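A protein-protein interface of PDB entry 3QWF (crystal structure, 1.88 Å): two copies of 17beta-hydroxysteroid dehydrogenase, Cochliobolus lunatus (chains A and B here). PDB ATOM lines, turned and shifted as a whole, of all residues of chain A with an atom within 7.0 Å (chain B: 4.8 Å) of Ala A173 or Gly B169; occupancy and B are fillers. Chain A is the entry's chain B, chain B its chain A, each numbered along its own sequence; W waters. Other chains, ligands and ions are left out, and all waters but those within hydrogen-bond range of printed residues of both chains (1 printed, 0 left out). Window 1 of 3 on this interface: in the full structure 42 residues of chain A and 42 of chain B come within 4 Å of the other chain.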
ATOM      1  N   PHE A 124     -21.700  15.502  -2.473  1.00  0.00           N
ATOM      2  CA  PHE A 124     -21.121  14.225  -2.053  1.00  0.00           C
ATOM      3  C   PHE A 124     -21.669  13.703  -0.718  1.00  0.00           C
ATOM      4  O   PHE A 124     -21.816  12.495  -0.557  1.00  0.00           O
ATOM      5  CB  PHE A 124     -19.591  14.304  -2.050  1.00  0.00           C
ATOM      6  CG  PHE A 124     -18.981  13.836  -3.339  1.00  0.00           C
ATOM      7  CD1 PHE A 124     -19.187  14.543  -4.520  1.00  0.00           C
ATOM      8  CD2 PHE A 124     -18.249  12.654  -3.386  1.00  0.00           C
ATOM      9  CE1 PHE A 124     -18.641  14.094  -5.730  1.00  0.00           C
ATOM     10  CE2 PHE A 124     -17.705  12.198  -4.587  1.00  0.00           C
ATOM     11  CZ  PHE A 124     -17.907  12.912  -5.760  1.00  0.00           C
ATOM     12  N   ASN A 127     -25.252  12.211  -1.998  1.00  0.00           N
ATOM     13  CA  ASN A 127     -25.217  11.318  -3.169  1.00  0.00           C
ATOM     14  C   ASN A 127     -24.278  10.136  -3.046  1.00  0.00           C
ATOM     15  O   ASN A 127     -24.500   9.092  -3.653  1.00  0.00           O
ATOM     16  CB  ASN A 127     -24.830  12.106  -4.427  1.00  0.00           C
ATOM     17  CG  ASN A 127     -25.894  13.097  -4.845  1.00  0.00           C
ATOM     18  OD1 ASN A 127     -26.834  13.380  -4.095  1.00  0.00           O
ATOM     19  ND2 ASN A 127     -25.747  13.642  -6.047  1.00  0.00           N
ATOM     20  N   THR A 128     -23.220  10.320  -2.265  1.00  0.00           N
ATOM     21  CA  THR A 128     -22.094   9.409  -2.265  1.00  0.00           C
ATOM     22  C   THR A 128     -21.823   8.894  -0.855  1.00  0.00           C
ATOM     23  O   THR A 128     -21.934   7.679  -0.603  1.00  0.00           O
ATOM     24  CB  THR A 128     -20.861  10.121  -2.850  1.00  0.00           C
ATOM     25  OG1 THR A 128     -21.228  10.705  -4.106  1.00  0.00           O
ATOM     26  CG2 THR A 128     -19.719   9.132  -3.063  1.00  0.00           C
ATOM     27  N   SER A 152     -27.683   5.579  -9.064  1.00  0.00           N
ATOM     28  CA  SER A 152     -26.636   6.247  -9.814  1.00  0.00           C
ATOM     29  C   SER A 152     -27.321   7.155 -10.841  1.00  0.00           C
ATOM     30  O   SER A 152     -28.357   7.754 -10.544  1.00  0.00           O
ATOM     31  CB  SER A 152     -25.754   5.186 -10.482  1.00  0.00           C
ATOM     32  OG  SER A 152     -24.703   5.782 -11.230  1.00  0.00           O
ATOM     33  N   SER A 156     -23.200   9.134 -14.873  1.00  0.00           N
ATOM     34  CA  SER A 156     -22.015   8.516 -14.288  1.00  0.00           C
ATOM     35  C   SER A 156     -21.012   8.080 -15.370  1.00  0.00           C
ATOM     36  O   SER A 156     -19.848   8.523 -15.358  1.00  0.00           O
ATOM     37  CB  SER A 156     -22.409   7.343 -13.399  1.00  0.00           C
ATOM     38  OG  SER A 156     -21.248   6.602 -13.059  1.00  0.00           O
ATOM     39  N   LYS A 157     -21.478   7.241 -16.303  1.00  0.00           N
ATOM     40  CA  LYS A 157     -20.644   6.667 -17.369  1.00  0.00           C
ATOM     41  C   LYS A 157     -21.172   6.860 -18.788  1.00  0.00           C
ATOM     42  O   LYS A 157     -20.383   6.979 -19.718  1.00  0.00           O
ATOM     43  CB  LYS A 157     -20.464   5.160 -17.169  1.00  0.00           C
ATOM     44  CG  LYS A 157     -19.664   4.803 -15.956  1.00  0.00           C
ATOM     45  CD  LYS A 157     -19.623   3.293 -15.689  1.00  0.00           C
ATOM     46  CE  LYS A 157     -18.735   3.055 -14.449  1.00  0.00           C
ATOM     47  NZ  LYS A 157     -18.869   4.169 -13.415  1.00  0.00           N
ATOM     48  N   SER A 168     -21.826  13.966 -11.823  1.00  0.00           N
ATOM     49  CA  SER A 168     -21.440  12.718 -12.522  1.00  0.00           C
ATOM     50  C   SER A 168     -20.473  11.876 -11.693  1.00  0.00           C
ATOM     51  O   SER A 168     -20.616  10.630 -11.617  1.00  0.00           O
ATOM     52  CB  SER A 168     -20.827  13.012 -13.895  1.00  0.00           C
ATOM     53  OG  SER A 168     -21.701  13.794 -14.702  1.00  0.00           O
ATOM     54  N   GLY A 169     -19.476  12.553 -11.110  1.00  0.00           N
ATOM     55  CA  GLY A 169     -18.517  11.927 -10.187  1.00  0.00           C
ATOM     56  C   GLY A 169     -19.162  11.324  -8.946  1.00  0.00           C
ATOM     57  O   GLY A 169     -18.786  10.225  -8.506  1.00  0.00           O
ATOM     58  N   SER A 170     -20.137  12.032  -8.386  1.00  0.00           N
ATOM     59  CA  SER A 170     -20.871  11.555  -7.203  1.00  0.00           C
ATOM     60  C   SER A 170     -21.521  10.187  -7.444  1.00  0.00           C
ATOM     61  O   SER A 170     -21.553   9.333  -6.542  1.00  0.00           O
ATOM     62  CB  SER A 170     -21.887  12.601  -6.711  1.00  0.00           C
ATOM     63  OG  SER A 170     -23.125  12.551  -7.404  1.00  0.00           O
ATOM     64  N   LYS A 171     -22.001   9.972  -8.664  1.00  0.00           N
ATOM     65  CA  LYS A 171     -22.632   8.699  -9.024  1.00  0.00           C
ATOM     66  C   LYS A 171     -21.615   7.696  -9.548  1.00  0.00           C
ATOM     67  O   LYS A 171     -21.817   6.498  -9.407  1.00  0.00           O
ATOM     68  CB  LYS A 171     -23.790   8.903 -10.032  1.00  0.00           C
ATOM     69  CG  LYS A 171     -24.879   9.886  -9.571  1.00  0.00           C
ATOM     70  CD  LYS A 171     -25.302   9.664  -8.102  1.00  0.00           C
ATOM     71  CE  LYS A 171     -26.517  10.519  -7.736  1.00  0.00           C
ATOM     72  NZ  LYS A 171     -27.798   9.971  -8.308  1.00  0.00           N
ATOM     73  N   GLY A 172     -20.517   8.170 -10.149  1.00  0.00           N
ATOM     74  CA  GLY A 172     -19.416   7.258 -10.520  1.00  0.00           C
ATOM     75  C   GLY A 172     -18.894   6.481  -9.316  1.00  0.00           C
ATOM     76  O   GLY A 172     -18.596   5.280  -9.404  1.00  0.00           O
ATOM     77  N   ALA A 173     -18.822   7.156  -8.168  1.00  0.00           N
ATOM     78  CA  ALA A 173     -18.377   6.480  -6.944  1.00  0.00           C
ATOM     79  C   ALA A 173     -19.346   5.347  -6.564  1.00  0.00           C
ATOM     80  O   ALA A 173     -18.923   4.248  -6.190  1.00  0.00           O
ATOM     81  CB  ALA A 173     -18.221   7.509  -5.789  1.00  0.00           C
ATOM     82  N   VAL A 174     -20.641   5.626  -6.688  1.00  0.00           N
ATOM     83  CA  VAL A 174     -21.715   4.655  -6.408  1.00  0.00           C
ATOM     84  C   VAL A 174     -21.609   3.402  -7.289  1.00  0.00           C
ATOM     85  O   VAL A 174     -21.736   2.278  -6.801  1.00  0.00           O
ATOM     86  CB  VAL A 174     -23.124   5.333  -6.538  1.00  0.00           C
ATOM     87  CG1 VAL A 174     -24.271   4.312  -6.450  1.00  0.00           C
ATOM     88  CG2 VAL A 174     -23.282   6.424  -5.470  1.00  0.00           C
ATOM     89  N   ASP A 175     -21.342   3.585  -8.574  1.00  0.00           N
ATOM     90  CA  ASP A 175     -21.148   2.443  -9.490  1.00  0.00           C
ATOM     91  C   ASP A 175     -20.068   1.495  -8.965  1.00  0.00           C
ATOM     92  O   ASP A 175     -20.238   0.259  -8.963  1.00  0.00           O
ATOM     93  CB  ASP A 175     -20.740   2.942 -10.877  1.00  0.00           C
ATOM     94  CG  ASP A 175     -21.859   3.706 -11.585  1.00  0.00           C
ATOM     95  OD1 ASP A 175     -22.964   3.864 -11.020  1.00  0.00           O
ATOM     96  OD2 ASP A 175     -21.617   4.141 -12.721  1.00  0.00           O
ATOM     97  N   SER A 176     -18.949   2.075  -8.543  1.00  0.00           N
ATOM     98  CA  SER A 176     -17.842   1.286  -8.008  1.00  0.00           C
ATOM     99  C   SER A 176     -18.240   0.672  -6.660  1.00  0.00           C
ATOM    100  O   SER A 176     -17.983  -0.518  -6.407  1.00  0.00           O
ATOM    101  CB  SER A 176     -16.569   2.135  -7.905  1.00  0.00           C
ATOM    102  OG  SER A 176     -16.043   2.398  -9.207  1.00  0.00           O
ATOM    103  N   PHE A 177     -18.914   1.455  -5.819  1.00  0.00           N
ATOM    104  CA  PHE A 177     -19.371   0.947  -4.521  1.00  0.00           C
ATOM    105  C   PHE A 177     -20.155  -0.370  -4.659  1.00  0.00           C
ATOM    106  O   PHE A 177     -19.801  -1.399  -4.032  1.00  0.00           O
ATOM    107  CB  PHE A 177     -20.269   1.955  -3.789  1.00  0.00           C
ATOM    108  CG  PHE A 177     -19.558   3.143  -3.184  1.00  0.00           C
ATOM    109  CD1 PHE A 177     -18.195   3.117  -2.846  1.00  0.00           C
ATOM    110  CD2 PHE A 177     -20.302   4.288  -2.890  1.00  0.00           C
ATOM    111  CE1 PHE A 177     -17.578   4.259  -2.251  1.00  0.00           C
ATOM    112  CE2 PHE A 177     -19.714   5.424  -2.284  1.00  0.00           C
ATOM    113  CZ  PHE A 177     -18.350   5.413  -1.968  1.00  0.00           C
ATOM    114  N   VAL A 178     -21.213  -0.363  -5.473  1.00  0.00           N
ATOM    115  CA  VAL A 178     -22.102  -1.540  -5.524  1.00  0.00           C
ATOM    116  C   VAL A 178     -21.414  -2.814  -5.982  1.00  0.00           C
ATOM    117  O   VAL A 178     -21.760  -3.906  -5.501  1.00  0.00           O
ATOM    118  CB  VAL A 178     -23.421  -1.315  -6.343  1.00  0.00           C
ATOM    119  CG1 VAL A 178     -24.204  -0.128  -5.774  1.00  0.00           C
ATOM    120  CG2 VAL A 178     -23.147  -1.166  -7.816  1.00  0.00           C
ATOM    121  N   ILE A 180     -18.372  -3.754  -5.378  1.00  0.00           N
ATOM    122  CA  ILE A 180     -17.558  -4.307  -4.283  1.00  0.00           C
ATOM    123  C   ILE A 180     -18.460  -4.632  -3.079  1.00  0.00           C
ATOM    124  O   ILE A 180     -18.228  -5.610  -2.359  1.00  0.00           O
ATOM    125  CB  ILE A 180     -16.381  -3.361  -3.909  1.00  0.00           C
ATOM    126  CG1 ILE A 180     -15.593  -2.908  -5.168  1.00  0.00           C
ATOM    127  CG2 ILE A 180     -15.460  -4.014  -2.858  1.00  0.00           C
ATOM    128  CD1 ILE A 180     -15.146  -4.025  -6.107  1.00  0.00           C
ATOM    129  N   PHE B 124     -11.790   9.816   1.055  1.00  0.00           N
ATOM    130  CA  PHE B 124     -12.390  10.745   0.073  1.00  0.00           C
ATOM    131  C   PHE B 124     -11.816  12.174   0.040  1.00  0.00           C
ATOM    132  O   PHE B 124     -11.718  12.780  -1.041  1.00  0.00           O
ATOM    133  CB  PHE B 124     -13.920  10.763   0.193  1.00  0.00           C
ATOM    134  CG  PHE B 124     -14.602   9.804  -0.748  1.00  0.00           C
ATOM    135  CD1 PHE B 124     -14.486   8.426  -0.554  1.00  0.00           C
ATOM    136  CD2 PHE B 124     -15.325  10.269  -1.843  1.00  0.00           C
ATOM    137  CE1 PHE B 124     -15.099   7.523  -1.417  1.00  0.00           C
ATOM    138  CE2 PHE B 124     -15.953   9.366  -2.732  1.00  0.00           C
ATOM    139  CZ  PHE B 124     -15.834   7.977  -2.506  1.00  0.00           C
ATOM    140  N   SER B 165     -14.304  -1.535  -1.054  1.00  0.00           N
ATOM    141  CA  SER B 165     -15.388  -0.710  -1.617  1.00  0.00           C
ATOM    142  C   SER B 165     -15.080   0.771  -1.506  1.00  0.00           C
ATOM    143  O   SER B 165     -15.236   1.518  -2.479  1.00  0.00           O
ATOM    144  CB  SER B 165     -16.753  -1.041  -0.986  1.00  0.00           C
ATOM    145  OG  SER B 165     -16.830  -0.709   0.399  1.00  0.00           O
ATOM    146  N   LEU B 166     -14.592   1.179  -0.334  1.00  0.00           N
ATOM    147  CA  LEU B 166     -14.331   2.596  -0.081  1.00  0.00           C
ATOM    148  C   LEU B 166     -13.307   3.166  -1.062  1.00  0.00           C
ATOM    149  O   LEU B 166     -13.553   4.190  -1.690  1.00  0.00           O
ATOM    150  CB  LEU B 166     -13.899   2.841   1.375  1.00  0.00           C
ATOM    151  CG  LEU B 166     -13.484   4.291   1.702  1.00  0.00           C
ATOM    152  CD1 LEU B 166     -14.640   5.243   1.450  1.00  0.00           C
ATOM    153  CD2 LEU B 166     -12.981   4.446   3.129  1.00  0.00           C
ATOM    154  N   TYR B 167     -12.154   2.515  -1.182  1.00  0.00           N
ATOM    155  CA  TYR B 167     -11.117   3.017  -2.083  1.00  0.00           C
ATOM    156  C   TYR B 167     -11.567   2.912  -3.560  1.00  0.00           C
ATOM    157  O   TYR B 167     -11.273   3.808  -4.383  1.00  0.00           O
ATOM    158  CB  TYR B 167      -9.834   2.223  -1.854  1.00  0.00           C
ATOM    159  CG  TYR B 167      -8.704   2.547  -2.804  1.00  0.00           C
ATOM    160  CD1 TYR B 167      -8.559   1.863  -4.009  1.00  0.00           C
ATOM    161  CD2 TYR B 167      -7.756   3.523  -2.476  1.00  0.00           C
ATOM    162  CE1 TYR B 167      -7.497   2.150  -4.870  1.00  0.00           C
ATOM    163  CE2 TYR B 167      -6.707   3.816  -3.319  1.00  0.00           C
ATOM    164  CZ  TYR B 167      -6.585   3.130  -4.515  1.00  0.00           C
ATOM    165  OH  TYR B 167      -5.535   3.410  -5.342  1.00  0.00           O
ATOM    166  N   SER B 168     -12.224   1.800  -3.904  1.00  0.00           N
ATOM    167  CA  SER B 168     -12.665   1.566  -5.291  1.00  0.00           C
ATOM    168  C   SER B 168     -13.598   2.694  -5.730  1.00  0.00           C
ATOM    169  O   SER B 168     -13.417   3.247  -6.808  1.00  0.00           O
ATOM    170  CB  SER B 168     -13.342   0.198  -5.483  1.00  0.00           C
ATOM    171  OG  SER B 168     -12.480  -0.880  -5.124  1.00  0.00           O
ATOM    172  N   GLY B 169     -14.559   3.045  -4.872  1.00  0.00           N
ATOM    173  CA  GLY B 169     -15.448   4.181  -5.127  1.00  0.00           C
ATOM    174  C   GLY B 169     -14.775   5.544  -5.177  1.00  0.00           C
ATOM    175  O   GLY B 169     -15.204   6.436  -5.931  1.00  0.00           O
ATOM    176  N   SER B 170     -13.720   5.741  -4.379  1.00  0.00           N
ATOM    177  CA  SER B 170     -13.033   7.048  -4.404  1.00  0.00           C
ATOM    178  C   SER B 170     -12.418   7.299  -5.786  1.00  0.00           C
ATOM    179  O   SER B 170     -12.329   8.449  -6.255  1.00  0.00           O
ATOM    180  CB  SER B 170     -11.984   7.167  -3.272  1.00  0.00           C
ATOM    181  OG  SER B 170     -10.793   6.440  -3.563  1.00  0.00           O
ATOM    182  N   LYS B 171     -12.030   6.218  -6.459  1.00  0.00           N
ATOM    183  CA  LYS B 171     -11.412   6.330  -7.791  1.00  0.00           C
ATOM    184  C   LYS B 171     -12.459   6.279  -8.924  1.00  0.00           C
ATOM    185  O   LYS B 171     -12.247   6.841 -10.002  1.00  0.00           O
ATOM    186  CB  LYS B 171     -10.311   5.263  -7.950  1.00  0.00           C
ATOM    187  CG  LYS B 171      -9.181   5.401  -6.874  1.00  0.00           C
ATOM    188  CD  LYS B 171      -8.684   6.891  -6.719  1.00  0.00           C
ATOM    189  CE  LYS B 171      -7.416   7.007  -5.858  1.00  0.00           C
ATOM    190  NZ  LYS B 171      -6.184   6.597  -6.599  1.00  0.00           N
ATOM    191  N   GLY B 172     -13.595   5.633  -8.671  1.00  0.00           N
ATOM    192  CA  GLY B 172     -14.712   5.616  -9.632  1.00  0.00           C
ATOM    193  C   GLY B 172     -15.246   7.028  -9.870  1.00  0.00           C
ATOM    194  O   GLY B 172     -15.602   7.380 -10.991  1.00  0.00           O
ATOM    195  N   ALA B 173     -15.290   7.836  -8.818  1.00  0.00           N
ATOM    196  CA  ALA B 173     -15.622   9.263  -8.929  1.00  0.00           C
ATOM    197  C   ALA B 173     -14.647   9.989  -9.856  1.00  0.00           C
ATOM    198  O   ALA B 173     -15.063  10.779 -10.708  1.00  0.00           O
ATOM    199  CB  ALA B 173     -15.624   9.922  -7.555  1.00  0.00           C
HETATM  200  O   HOH W   1     -17.160   6.210 -13.865  1.00  0.00           O
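Water W1 bridges the side-chain amino group of Lys A157 and the backbone carbonyl oxygen of Gly B172.
Of chain B, only Gly B169 (3.2 Å), Gly B172 (3.96 Å) and Ala B173 (3.7 Å) come within 4 Å of Ala A173.
Of the printed residues of chain A, Gly B169 touches Ala A173 (3.2 Å), Ser A176 (3.6 Å) and Phe A177 (3.6 Å).
Printed residues of chain A within 4 Å of Phe B124: Phe A124, Thr A128 and Phe A177.
Printed residues of chain A within 4 Å of Ser B165: Phe A177 and Ile A180.
Of the printed residues of chain B, Ile A180 touches Ser B165 and Ser B168.
Ser A152 touches none of the printed residues of chain B.
Ser A170 touches none of the printed residues of chain B.
The nearest residue of chain B that does not touch Ala A173 is Phe B124 (4.1 Å).
The nearest residue of chain A that does not touch Gly B169 is Gly A172 (5.0 Å).
Hydrophobic or aromatic side chains of chain B within 4 Å of the printed part of chain A: Phe B124 and Ala B173.
Hydrophobic or aromatic side chains of chain A that line the printed part of chain B: Phe A124, Ala A173, Phe A177 and Ile A180.
Among the printed residues, 16 pairs touch across the chains.
The backbone carbonyl oxygen of Ser A170 is in hydrogen-bond range of the side-chain hydroxyl of Thr A128, 2.8 Å away.
The side-chain hydroxyl of Ser A156 sits close to the backbone NH of Gly A172, 3.4 Å away.
Among the printed residues, pairs that only touch across the chains: Phe A124 with Phe B124 (3.8 Å), Thr A128 with Phe B124 (3.8 Å), Gly A169 with Ala B173 (3.3 Å), Gly A172 with Gly B172 (3.7 Å), Gly A172 with Ala B173 (3.9 Å), Ala A173 with Gly B169 (3.2 Å), Ala A173 with Gly B172 (3.96 Å), Ala A173 with Ala B173 (3.7 Å), Ser A176 with Ser B168 (3.5 Å), Ser A176 with Gly B169 (3.6 Å), Ser A176 with Gly B172 (3.5 Å), Phe A177 with Phe B124 (3.6 Å), Phe A177 with Ser B165 (3.4 Å), Phe A177 with Gly B169 (3.6 Å), Ile A180 with Ser B165 (3.3 Å) and Ile A180 with Ser B168 (3.7 Å).
Phe B124 touches its own counterpart, Phe A124.
Gly A169 touches Ala B173, and with the chains exchanged Ala A173 touches Gly B169.
Gly B172 touches its own counterpart, Gly A172.
Gly A172 touches Ala B173, and with the chains exchanged Ala A173 touches Gly B172.
Positions printed for both chains: 124, 168, 169, 170, 171, 172 and 173.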
